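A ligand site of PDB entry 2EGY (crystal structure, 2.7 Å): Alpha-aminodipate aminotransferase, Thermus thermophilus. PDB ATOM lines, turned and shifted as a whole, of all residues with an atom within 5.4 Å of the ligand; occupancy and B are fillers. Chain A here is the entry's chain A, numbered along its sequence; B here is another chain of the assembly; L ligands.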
ATOM      1  N   THR A  98      21.820 -17.385 -12.418  1.00  0.00           N
ATOM      2  CA  THR A  98      20.653 -16.588 -12.104  1.00  0.00           C
ATOM      3  C   THR A  98      20.871 -16.054 -10.686  1.00  0.00           C
ATOM      4  O   THR A  98      20.306 -16.563  -9.712  1.00  0.00           O
ATOM      5  CB  THR A  98      19.388 -17.447 -12.172  1.00  0.00           C
ATOM      6  OG1 THR A  98      19.312 -18.047 -13.478  1.00  0.00           O
ATOM      7  CG2 THR A  98      18.129 -16.601 -11.925  1.00  0.00           C
ATOM      8  N   GLY A  99      21.717 -15.042 -10.584  1.00  0.00           N
ATOM      9  CA  GLY A  99      22.028 -14.439  -9.297  1.00  0.00           C
ATOM     10  C   GLY A  99      23.048 -15.294  -8.590  1.00  0.00           C
ATOM     11  O   GLY A  99      23.220 -16.466  -8.939  1.00  0.00           O
ATOM     12  N   SER A 100      23.763 -14.718  -7.627  1.00  0.00           N
ATOM     13  CA  SER A 100      24.721 -15.498  -6.873  1.00  0.00           C
ATOM     14  C   SER A 100      23.959 -16.567  -6.106  1.00  0.00           C
ATOM     15  O   SER A 100      24.464 -17.659  -5.845  1.00  0.00           O
ATOM     16  CB  SER A 100      25.491 -14.607  -5.918  1.00  0.00           C
ATOM     17  OG  SER A 100      26.441 -13.847  -6.628  1.00  0.00           O
ATOM     18  N   GLN A 101      22.713 -16.256  -5.757  1.00  0.00           N
ATOM     19  CA  GLN A 101      21.898 -17.192  -5.012  1.00  0.00           C
ATOM     20  C   GLN A 101      21.957 -18.577  -5.628  1.00  0.00           C
ATOM     21  O   GLN A 101      21.960 -19.577  -4.911  1.00  0.00           O
ATOM     22  CB  GLN A 101      20.441 -16.729  -4.955  1.00  0.00           C
ATOM     23  CG  GLN A 101      19.606 -17.644  -4.095  1.00  0.00           C
ATOM     24  CD  GLN A 101      20.248 -17.891  -2.756  1.00  0.00           C
ATOM     25  OE1 GLN A 101      20.016 -18.919  -2.120  1.00  0.00           O
ATOM     26  NE2 GLN A 101      21.061 -16.942  -2.303  1.00  0.00           N
ATOM     27  N   GLN A 102      22.016 -18.644  -6.954  1.00  0.00           N
ATOM     28  CA  GLN A 102      22.096 -19.918  -7.642  1.00  0.00           C
ATOM     29  C   GLN A 102      23.457 -20.589  -7.479  1.00  0.00           C
ATOM     30  O   GLN A 102      23.530 -21.762  -7.120  1.00  0.00           O
ATOM     31  CB  GLN A 102      21.805 -19.756  -9.123  1.00  0.00           C
ATOM     32  CG  GLN A 102      21.884 -21.069  -9.849  1.00  0.00           C
ATOM     33  CD  GLN A 102      21.333 -20.994 -11.250  1.00  0.00           C
ATOM     34  OE1 GLN A 102      21.989 -20.485 -12.160  1.00  0.00           O
ATOM     35  NE2 GLN A 102      20.115 -21.485 -11.426  1.00  0.00           N
ATOM     36  N   LEU A 104      25.406 -20.510  -5.253  1.00  0.00           N
ATOM     37  CA  LEU A 104      25.513 -21.077  -3.908  1.00  0.00           C
ATOM     38  C   LEU A 104      24.713 -22.365  -3.880  1.00  0.00           C
ATOM     39  O   LEU A 104      24.982 -23.263  -3.072  1.00  0.00           O
ATOM     40  CB  LEU A 104      24.953 -20.108  -2.866  1.00  0.00           C
ATOM     41  CG  LEU A 104      25.612 -18.741  -2.713  1.00  0.00           C
ATOM     42  CD1 LEU A 104      24.747 -17.889  -1.802  1.00  0.00           C
ATOM     43  CD2 LEU A 104      26.989 -18.881  -2.158  1.00  0.00           C
ATOM     44  N   TYR A 125      26.046 -14.960   5.605  1.00  0.00           N
ATOM     45  CA  TYR A 125      24.905 -14.744   4.726  1.00  0.00           C
ATOM     46  C   TYR A 125      23.825 -15.812   4.755  1.00  0.00           C
ATOM     47  O   TYR A 125      24.062 -16.959   4.388  1.00  0.00           O
ATOM     48  CB  TYR A 125      25.436 -14.573   3.300  1.00  0.00           C
ATOM     49  CG  TYR A 125      24.400 -14.400   2.230  1.00  0.00           C
ATOM     50  CD1 TYR A 125      23.295 -13.574   2.416  1.00  0.00           C
ATOM     51  CD2 TYR A 125      24.576 -15.004   0.997  1.00  0.00           C
ATOM     52  CE1 TYR A 125      22.391 -13.347   1.387  1.00  0.00           C
ATOM     53  CE2 TYR A 125      23.696 -14.781  -0.029  1.00  0.00           C
ATOM     54  CZ  TYR A 125      22.599 -13.950   0.168  1.00  0.00           C
ATOM     55  OH  TYR A 125      21.750 -13.749  -0.898  1.00  0.00           O
ATOM     56  N   TYR A 167      33.321 -21.114   2.985  1.00  0.00           N
ATOM     57  CA  TYR A 167      32.530 -20.038   2.372  1.00  0.00           C
ATOM     58  C   TYR A 167      32.850 -18.724   3.066  1.00  0.00           C
ATOM     59  O   TYR A 167      32.555 -18.549   4.245  1.00  0.00           O
ATOM     60  CB  TYR A 167      31.032 -20.333   2.498  1.00  0.00           C
ATOM     61  CG  TYR A 167      30.148 -19.148   2.112  1.00  0.00           C
ATOM     62  CD1 TYR A 167      30.028 -18.744   0.783  1.00  0.00           C
ATOM     63  CD2 TYR A 167      29.493 -18.403   3.088  1.00  0.00           C
ATOM     64  CE1 TYR A 167      29.270 -17.623   0.447  1.00  0.00           C
ATOM     65  CE2 TYR A 167      28.737 -17.286   2.761  1.00  0.00           C
ATOM     66  CZ  TYR A 167      28.625 -16.902   1.444  1.00  0.00           C
ATOM     67  OH  TYR A 167      27.890 -15.776   1.126  1.00  0.00           O
ATOM     68  N   ILE A 169      33.208 -14.158   2.738  1.00  0.00           N
ATOM     69  CA  ILE A 169      32.884 -12.895   2.094  1.00  0.00           C
ATOM     70  C   ILE A 169      33.916 -11.886   2.635  1.00  0.00           C
ATOM     71  O   ILE A 169      33.610 -11.066   3.500  1.00  0.00           O
ATOM     72  CB  ILE A 169      31.475 -12.426   2.497  1.00  0.00           C
ATOM     73  CG1 ILE A 169      30.529 -13.626   2.536  1.00  0.00           C
ATOM     74  CG2 ILE A 169      30.948 -11.419   1.493  1.00  0.00           C
ATOM     75  CD1 ILE A 169      29.171 -13.304   3.121  1.00  0.00           C
ATOM     76  N   ASN A 174      28.140  -9.914   4.770  1.00  0.00           N
ATOM     77  CA  ASN A 174      26.751  -9.752   5.153  1.00  0.00           C
ATOM     78  C   ASN A 174      26.738 -10.729   6.319  1.00  0.00           C
ATOM     79  O   ASN A 174      27.181 -11.848   6.151  1.00  0.00           O
ATOM     80  CB  ASN A 174      25.828 -10.260   4.041  1.00  0.00           C
ATOM     81  CG  ASN A 174      24.360 -10.109   4.374  1.00  0.00           C
ATOM     82  OD1 ASN A 174      23.986  -9.953   5.534  1.00  0.00           O
ATOM     83  ND2 ASN A 174      23.520 -10.176   3.353  1.00  0.00           N
ATOM     84  N   ASP A 202      32.562 -15.061  -2.048  1.00  0.00           N
ATOM     85  CA  ASP A 202      31.390 -14.285  -2.432  1.00  0.00           C
ATOM     86  C   ASP A 202      31.760 -12.795  -2.450  1.00  0.00           C
ATOM     87  O   ASP A 202      31.988 -12.204  -1.401  1.00  0.00           O
ATOM     88  CB  ASP A 202      30.284 -14.532  -1.413  1.00  0.00           C
ATOM     89  CG  ASP A 202      28.942 -14.007  -1.865  1.00  0.00           C
ATOM     90  OD1 ASP A 202      28.885 -12.952  -2.522  1.00  0.00           O
ATOM     91  OD2 ASP A 202      27.923 -14.648  -1.522  1.00  0.00           O
ATOM     92  N   ALA A 204      29.811 -10.091  -3.593  1.00  0.00           N
ATOM     93  CA  ALA A 204      28.638  -9.298  -3.948  1.00  0.00           C
ATOM     94  C   ALA A 204      28.918  -7.819  -3.789  1.00  0.00           C
ATOM     95  O   ALA A 204      28.372  -7.001  -4.508  1.00  0.00           O
ATOM     96  CB  ALA A 204      27.475  -9.675  -3.089  1.00  0.00           C
ATOM     97  N   TYR A 205      29.795  -7.481  -2.845  1.00  0.00           N
ATOM     98  CA  TYR A 205      30.126  -6.102  -2.551  1.00  0.00           C
ATOM     99  C   TYR A 205      31.497  -5.674  -3.056  1.00  0.00           C
ATOM    100  O   TYR A 205      32.060  -4.683  -2.584  1.00  0.00           O
ATOM    101  CB  TYR A 205      30.019  -5.878  -1.058  1.00  0.00           C
ATOM    102  CG  TYR A 205      28.649  -6.228  -0.533  1.00  0.00           C
ATOM    103  CD1 TYR A 205      27.571  -5.361  -0.739  1.00  0.00           C
ATOM    104  CD2 TYR A 205      28.403  -7.458   0.081  1.00  0.00           C
ATOM    105  CE1 TYR A 205      26.274  -5.700  -0.351  1.00  0.00           C
ATOM    106  CE2 TYR A 205      27.106  -7.812   0.484  1.00  0.00           C
ATOM    107  CZ  TYR A 205      26.050  -6.929   0.256  1.00  0.00           C
ATOM    108  OH  TYR A 205      24.767  -7.247   0.626  1.00  0.00           O
ATOM    109  N   SER A 235      28.195 -10.831  -8.467  1.00  0.00           N
ATOM    110  CA  SER A 235      26.844 -10.508  -8.854  1.00  0.00           C
ATOM    111  C   SER A 235      26.696  -9.145  -9.516  1.00  0.00           C
ATOM    112  O   SER A 235      27.642  -8.349  -9.563  1.00  0.00           O
ATOM    113  CB  SER A 235      25.925 -10.577  -7.658  1.00  0.00           C
ATOM    114  OG  SER A 235      24.657 -10.066  -7.990  1.00  0.00           O
ATOM    115  N   PHE A 236      25.503  -8.886 -10.039  1.00  0.00           N
ATOM    116  CA  PHE A 236      25.179  -7.623 -10.682  1.00  0.00           C
ATOM    117  C   PHE A 236      23.993  -7.037  -9.936  1.00  0.00           C
ATOM    118  O   PHE A 236      23.394  -6.061 -10.375  1.00  0.00           O
ATOM    119  CB  PHE A 236      24.789  -7.847 -12.149  1.00  0.00           C
ATOM    120  CG  PHE A 236      25.958  -7.996 -13.079  1.00  0.00           C
ATOM    121  CD1 PHE A 236      26.879  -6.956 -13.232  1.00  0.00           C
ATOM    122  CD2 PHE A 236      26.152  -9.166 -13.790  1.00  0.00           C
ATOM    123  CE1 PHE A 236      27.968  -7.098 -14.082  1.00  0.00           C
ATOM    124  CE2 PHE A 236      27.236  -9.317 -14.642  1.00  0.00           C
ATOM    125  CZ  PHE A 236      28.149  -8.273 -14.791  1.00  0.00           C
ATOM    126  N   SER A 237      23.670  -7.670  -8.812  1.00  0.00           N
ATOM    127  CA  SER A 237      22.533  -7.252  -7.992  1.00  0.00           C
ATOM    128  C   SER A 237      22.762  -6.011  -7.158  1.00  0.00           C
ATOM    129  O   SER A 237      21.810  -5.338  -6.776  1.00  0.00           O
ATOM    130  CB  SER A 237      22.126  -8.397  -7.066  1.00  0.00           C
ATOM    131  OG  SER A 237      21.648  -9.511  -7.790  1.00  0.00           O
ATOM    132  N   LYS A 238      24.023  -5.694  -6.864  1.00  0.00           N
ATOM    133  CA  LYS A 238      24.321  -4.530  -6.036  1.00  0.00           C
ATOM    134  C   LYS A 238      24.921  -3.359  -6.815  1.00  0.00           C
ATOM    135  O   LYS A 238      25.242  -2.316  -6.243  1.00  0.00           O
ATOM    136  CB  LYS A 238      25.272  -4.952  -4.910  1.00  0.00           C
ATOM    137  CG  LYS A 238      24.821  -6.199  -4.147  1.00  0.00           C
ATOM    138  CD  LYS A 238      23.656  -5.915  -3.195  1.00  0.00           C
ATOM    139  CE  LYS A 238      22.915  -7.195  -2.800  1.00  0.00           C
ATOM    140  NZ  LYS A 238      23.829  -8.315  -2.418  1.00  0.00           N
ATOM    141  N   PRO A 242      19.223  -5.983  -8.755  1.00  0.00           N
ATOM    142  CA  PRO A 242      19.116  -7.273  -8.093  1.00  0.00           C
ATOM    143  C   PRO A 242      18.006  -8.120  -8.713  1.00  0.00           C
ATOM    144  O   PRO A 242      18.115  -9.343  -8.786  1.00  0.00           O
ATOM    145  CB  PRO A 242      18.817  -6.895  -6.652  1.00  0.00           C
ATOM    146  CG  PRO A 242      18.001  -5.649  -6.809  1.00  0.00           C
ATOM    147  CD  PRO A 242      18.767  -4.895  -7.872  1.00  0.00           C
ATOM    148  N   ARG A 245      18.340 -10.759 -11.758  1.00  0.00           N
ATOM    149  CA  ARG A 245      18.852 -12.083 -11.392  1.00  0.00           C
ATOM    150  C   ARG A 245      19.958 -12.511 -12.342  1.00  0.00           C
ATOM    151  O   ARG A 245      19.882 -13.573 -12.966  1.00  0.00           O
ATOM    152  CB  ARG A 245      17.722 -13.125 -11.395  1.00  0.00           C
ATOM    153  CG  ARG A 245      16.442 -12.670 -10.709  1.00  0.00           C
ATOM    154  CD  ARG A 245      16.631 -12.286  -9.245  1.00  0.00           C
ATOM    155  NE  ARG A 245      17.146 -13.409  -8.475  1.00  0.00           N
ATOM    156  CZ  ARG A 245      18.312 -13.415  -7.840  1.00  0.00           C
ATOM    157  NH1 ARG A 245      19.084 -12.339  -7.859  1.00  0.00           N
ATOM    158  NH2 ARG A 245      18.707 -14.496  -7.187  1.00  0.00           N
ATOM    159  N   VAL A 246      20.978 -11.672 -12.459  1.00  0.00           N
ATOM    160  CA  VAL A 246      22.098 -11.971 -13.337  1.00  0.00           C
ATOM    161  C   VAL A 246      23.415 -11.865 -12.553  1.00  0.00           C
ATOM    162  O   VAL A 246      23.759 -10.799 -12.034  1.00  0.00           O
ATOM    163  CB  VAL A 246      22.123 -10.994 -14.528  1.00  0.00           C
ATOM    164  CG1 VAL A 246      23.241 -11.354 -15.497  1.00  0.00           C
ATOM    165  CG2 VAL A 246      20.785 -11.023 -15.229  1.00  0.00           C
ATOM    166  N   ALA A 247      24.127 -12.981 -12.470  1.00  0.00           N
ATOM    167  CA  ALA A 247      25.393 -13.006 -11.760  1.00  0.00           C
ATOM    168  C   ALA A 247      26.325 -13.975 -12.458  1.00  0.00           C
ATOM    169  O   ALA A 247      26.017 -14.471 -13.546  1.00  0.00           O
ATOM    170  CB  ALA A 247      25.163 -13.436 -10.322  1.00  0.00           C
ATOM    171  N   PHE A 326      25.394  -2.601   5.229  1.00  0.00           N
ATOM    172  CA  PHE A 326      24.829  -3.040   6.511  1.00  0.00           C
ATOM    173  C   PHE A 326      25.580  -2.494   7.709  1.00  0.00           C
ATOM    174  O   PHE A 326      26.691  -1.988   7.597  1.00  0.00           O
ATOM    175  CB  PHE A 326      24.847  -4.575   6.625  1.00  0.00           C
ATOM    176  CG  PHE A 326      24.124  -5.280   5.522  1.00  0.00           C
ATOM    177  CD1 PHE A 326      22.740  -5.307   5.481  1.00  0.00           C
ATOM    178  CD2 PHE A 326      24.837  -5.919   4.506  1.00  0.00           C
ATOM    179  CE1 PHE A 326      22.066  -5.951   4.445  1.00  0.00           C
ATOM    180  CE2 PHE A 326      24.180  -6.571   3.462  1.00  0.00           C
ATOM    181  CZ  PHE A 326      22.788  -6.585   3.440  1.00  0.00           C
ATOM    182  N   TYR B  70      14.532  -6.392  -5.964  1.00  0.00           N
ATOM    183  CA  TYR B  70      14.228  -7.725  -5.466  1.00  0.00           C
ATOM    184  C   TYR B  70      12.696  -7.781  -5.355  1.00  0.00           C
ATOM    185  O   TYR B  70      12.054  -6.785  -5.016  1.00  0.00           O
ATOM    186  CB  TYR B  70      14.844  -7.967  -4.085  1.00  0.00           C
ATOM    187  CG  TYR B  70      16.276  -8.424  -4.099  1.00  0.00           C
ATOM    188  CD1 TYR B  70      16.676  -9.484  -4.899  1.00  0.00           C
ATOM    189  CD2 TYR B  70      17.230  -7.841  -3.277  1.00  0.00           C
ATOM    190  CE1 TYR B  70      17.981  -9.970  -4.868  1.00  0.00           C
ATOM    191  CE2 TYR B  70      18.534  -8.318  -3.230  1.00  0.00           C
ATOM    192  CZ  TYR B  70      18.910  -9.375  -4.034  1.00  0.00           C
ATOM    193  OH  TYR B  70      20.183  -9.869  -3.986  1.00  0.00           O
ATOM    194  N   LEU B 268      16.294 -17.021  -5.155  1.00  0.00           N
ATOM    195  CA  LEU B 268      15.566 -15.940  -4.500  1.00  0.00           C
ATOM    196  C   LEU B 268      14.196 -15.738  -5.132  1.00  0.00           C
ATOM    197  O   LEU B 268      13.179 -15.868  -4.480  1.00  0.00           O
ATOM    198  CB  LEU B 268      16.371 -14.644  -4.527  1.00  0.00           C
ATOM    199  CG  LEU B 268      17.745 -14.668  -3.846  1.00  0.00           C
ATOM    200  CD1 LEU B 268      18.384 -13.303  -3.933  1.00  0.00           C
ATOM    201  CD2 LEU B 268      17.611 -15.088  -2.397  1.00  0.00           C
HETATM  202  N1  LIG L   1      26.086 -12.748  -1.497  1.00  0.00           N
HETATM  203  C1  LIG L   1      25.875 -11.815  -0.500  1.00  0.00           C
HETATM  204  C2  LIG L   1      26.666 -11.891   0.744  1.00  0.00           C
HETATM  205  C3  LIG L   1      24.935 -10.729  -0.722  1.00  0.00           C
HETATM  206  O1  LIG L   1      24.690  -9.825   0.284  1.00  0.00           O
HETATM  207  C4  LIG L   1      24.268 -10.620  -1.920  1.00  0.00           C
HETATM  208  C5  LIG L   1      23.354  -9.468  -2.133  1.00  0.00           C
HETATM  209  C6  LIG L   1      24.488 -11.574  -2.951  1.00  0.00           C
HETATM  210  C7  LIG L   1      25.412 -12.652  -2.721  1.00  0.00           C
HETATM  211  C8  LIG L   1      23.829 -11.405  -4.372  1.00  0.00           C
HETATM  212  O2  LIG L   1      22.840 -12.430  -4.607  1.00  0.00           O
HETATM  213  P1  LIG L   1      22.133 -12.476  -5.903  1.00  0.00           P
HETATM  214  O3  LIG L   1      20.938 -11.382  -5.906  1.00  0.00           O
HETATM  215  O4  LIG L   1      23.140 -12.147  -7.061  1.00  0.00           O
HETATM  216  O5  LIG L   1      21.523 -13.906  -6.118  1.00  0.00           O
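The side-chain amino group of Lys 238 is bonded to a carbon (C5) of the ligand, at 1.3 Å. OH of Tyr 70 of chain B lies within hydrogen-bond range of O3 of the ligand (2.6 Å). An oxygen (O1) of the ligand sits at hydrogen-bond distance from the side-chain hydroxyl of Tyr 205. OD2 of Asp 202 is in hydrogen-bond range of N1 of the ligand. The backbone NH (N) of Gln 101 lies within hydrogen-bond range of an oxygen (O5) of the ligand, at 2.7 Å. The backbone NH (N) of Ser 100 is in hydrogen-bond range of an oxygen (O4) of the ligand (2.7 Å). OG of Ser 235 sits at hydrogen-bond distance from O4 of the ligand (2.7 Å). OG of Ser 237 lies within hydrogen-bond range of O3 of the ligand (2.7 Å). The guanidinium group (NH1) of Arg 245 is in salt-bridge range of an oxygen (O3) of the ligand (2.9 Å). ND2 of Asn 174 lies within hydrogen-bond range of O1 of the ligand (3.3 Å).
Gly 99 touches the ligand (C to O5, 3.2 Å). Tyr 125 touches the ligand (CE2 to N1, 3.5 Å). Ile 169 touches the ligand (CD1 to C2, 3.7 Å). CB of Ala 204 touches C4 of the ligand (3.5 Å). CD1 of Leu 268 of chain B touches O3 of the ligand (3.8 Å). Hydrophobic or aromatic side chains within 4 Å of the ligand: Tyr 125, Ile 169, Ala 204, Tyr 205, Tyr 70 of chain B and Leu 268 of chain B. Along chain A the residues within 4 Å of the ligand span positions 99 to 245.
OH of Tyr 205 is in hydrogen-bond range of NZ of Lys 238 (3.4 Å). N of Ala 204 lies within hydrogen-bond range of OD1 of Asp 202. The side-chain carboxylate (OD2) of Asp 202 sits at hydrogen-bond distance from the side-chain hydroxyl (OH) of Tyr 167. N of Ser 237 lies within hydrogen-bond range of OG of Ser 235. The backbone NH of Gly 99 lies within hydrogen-bond range of the backbone carbonyl oxygen of Arg 245. The guanidinium group of Arg 245 lies within hydrogen-bond range of the backbone carbonyl oxygen of Pro 242 (3.3 Å). O of Asn 174 is in hydrogen-bond range of N of Tyr 125 (3.4 Å).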
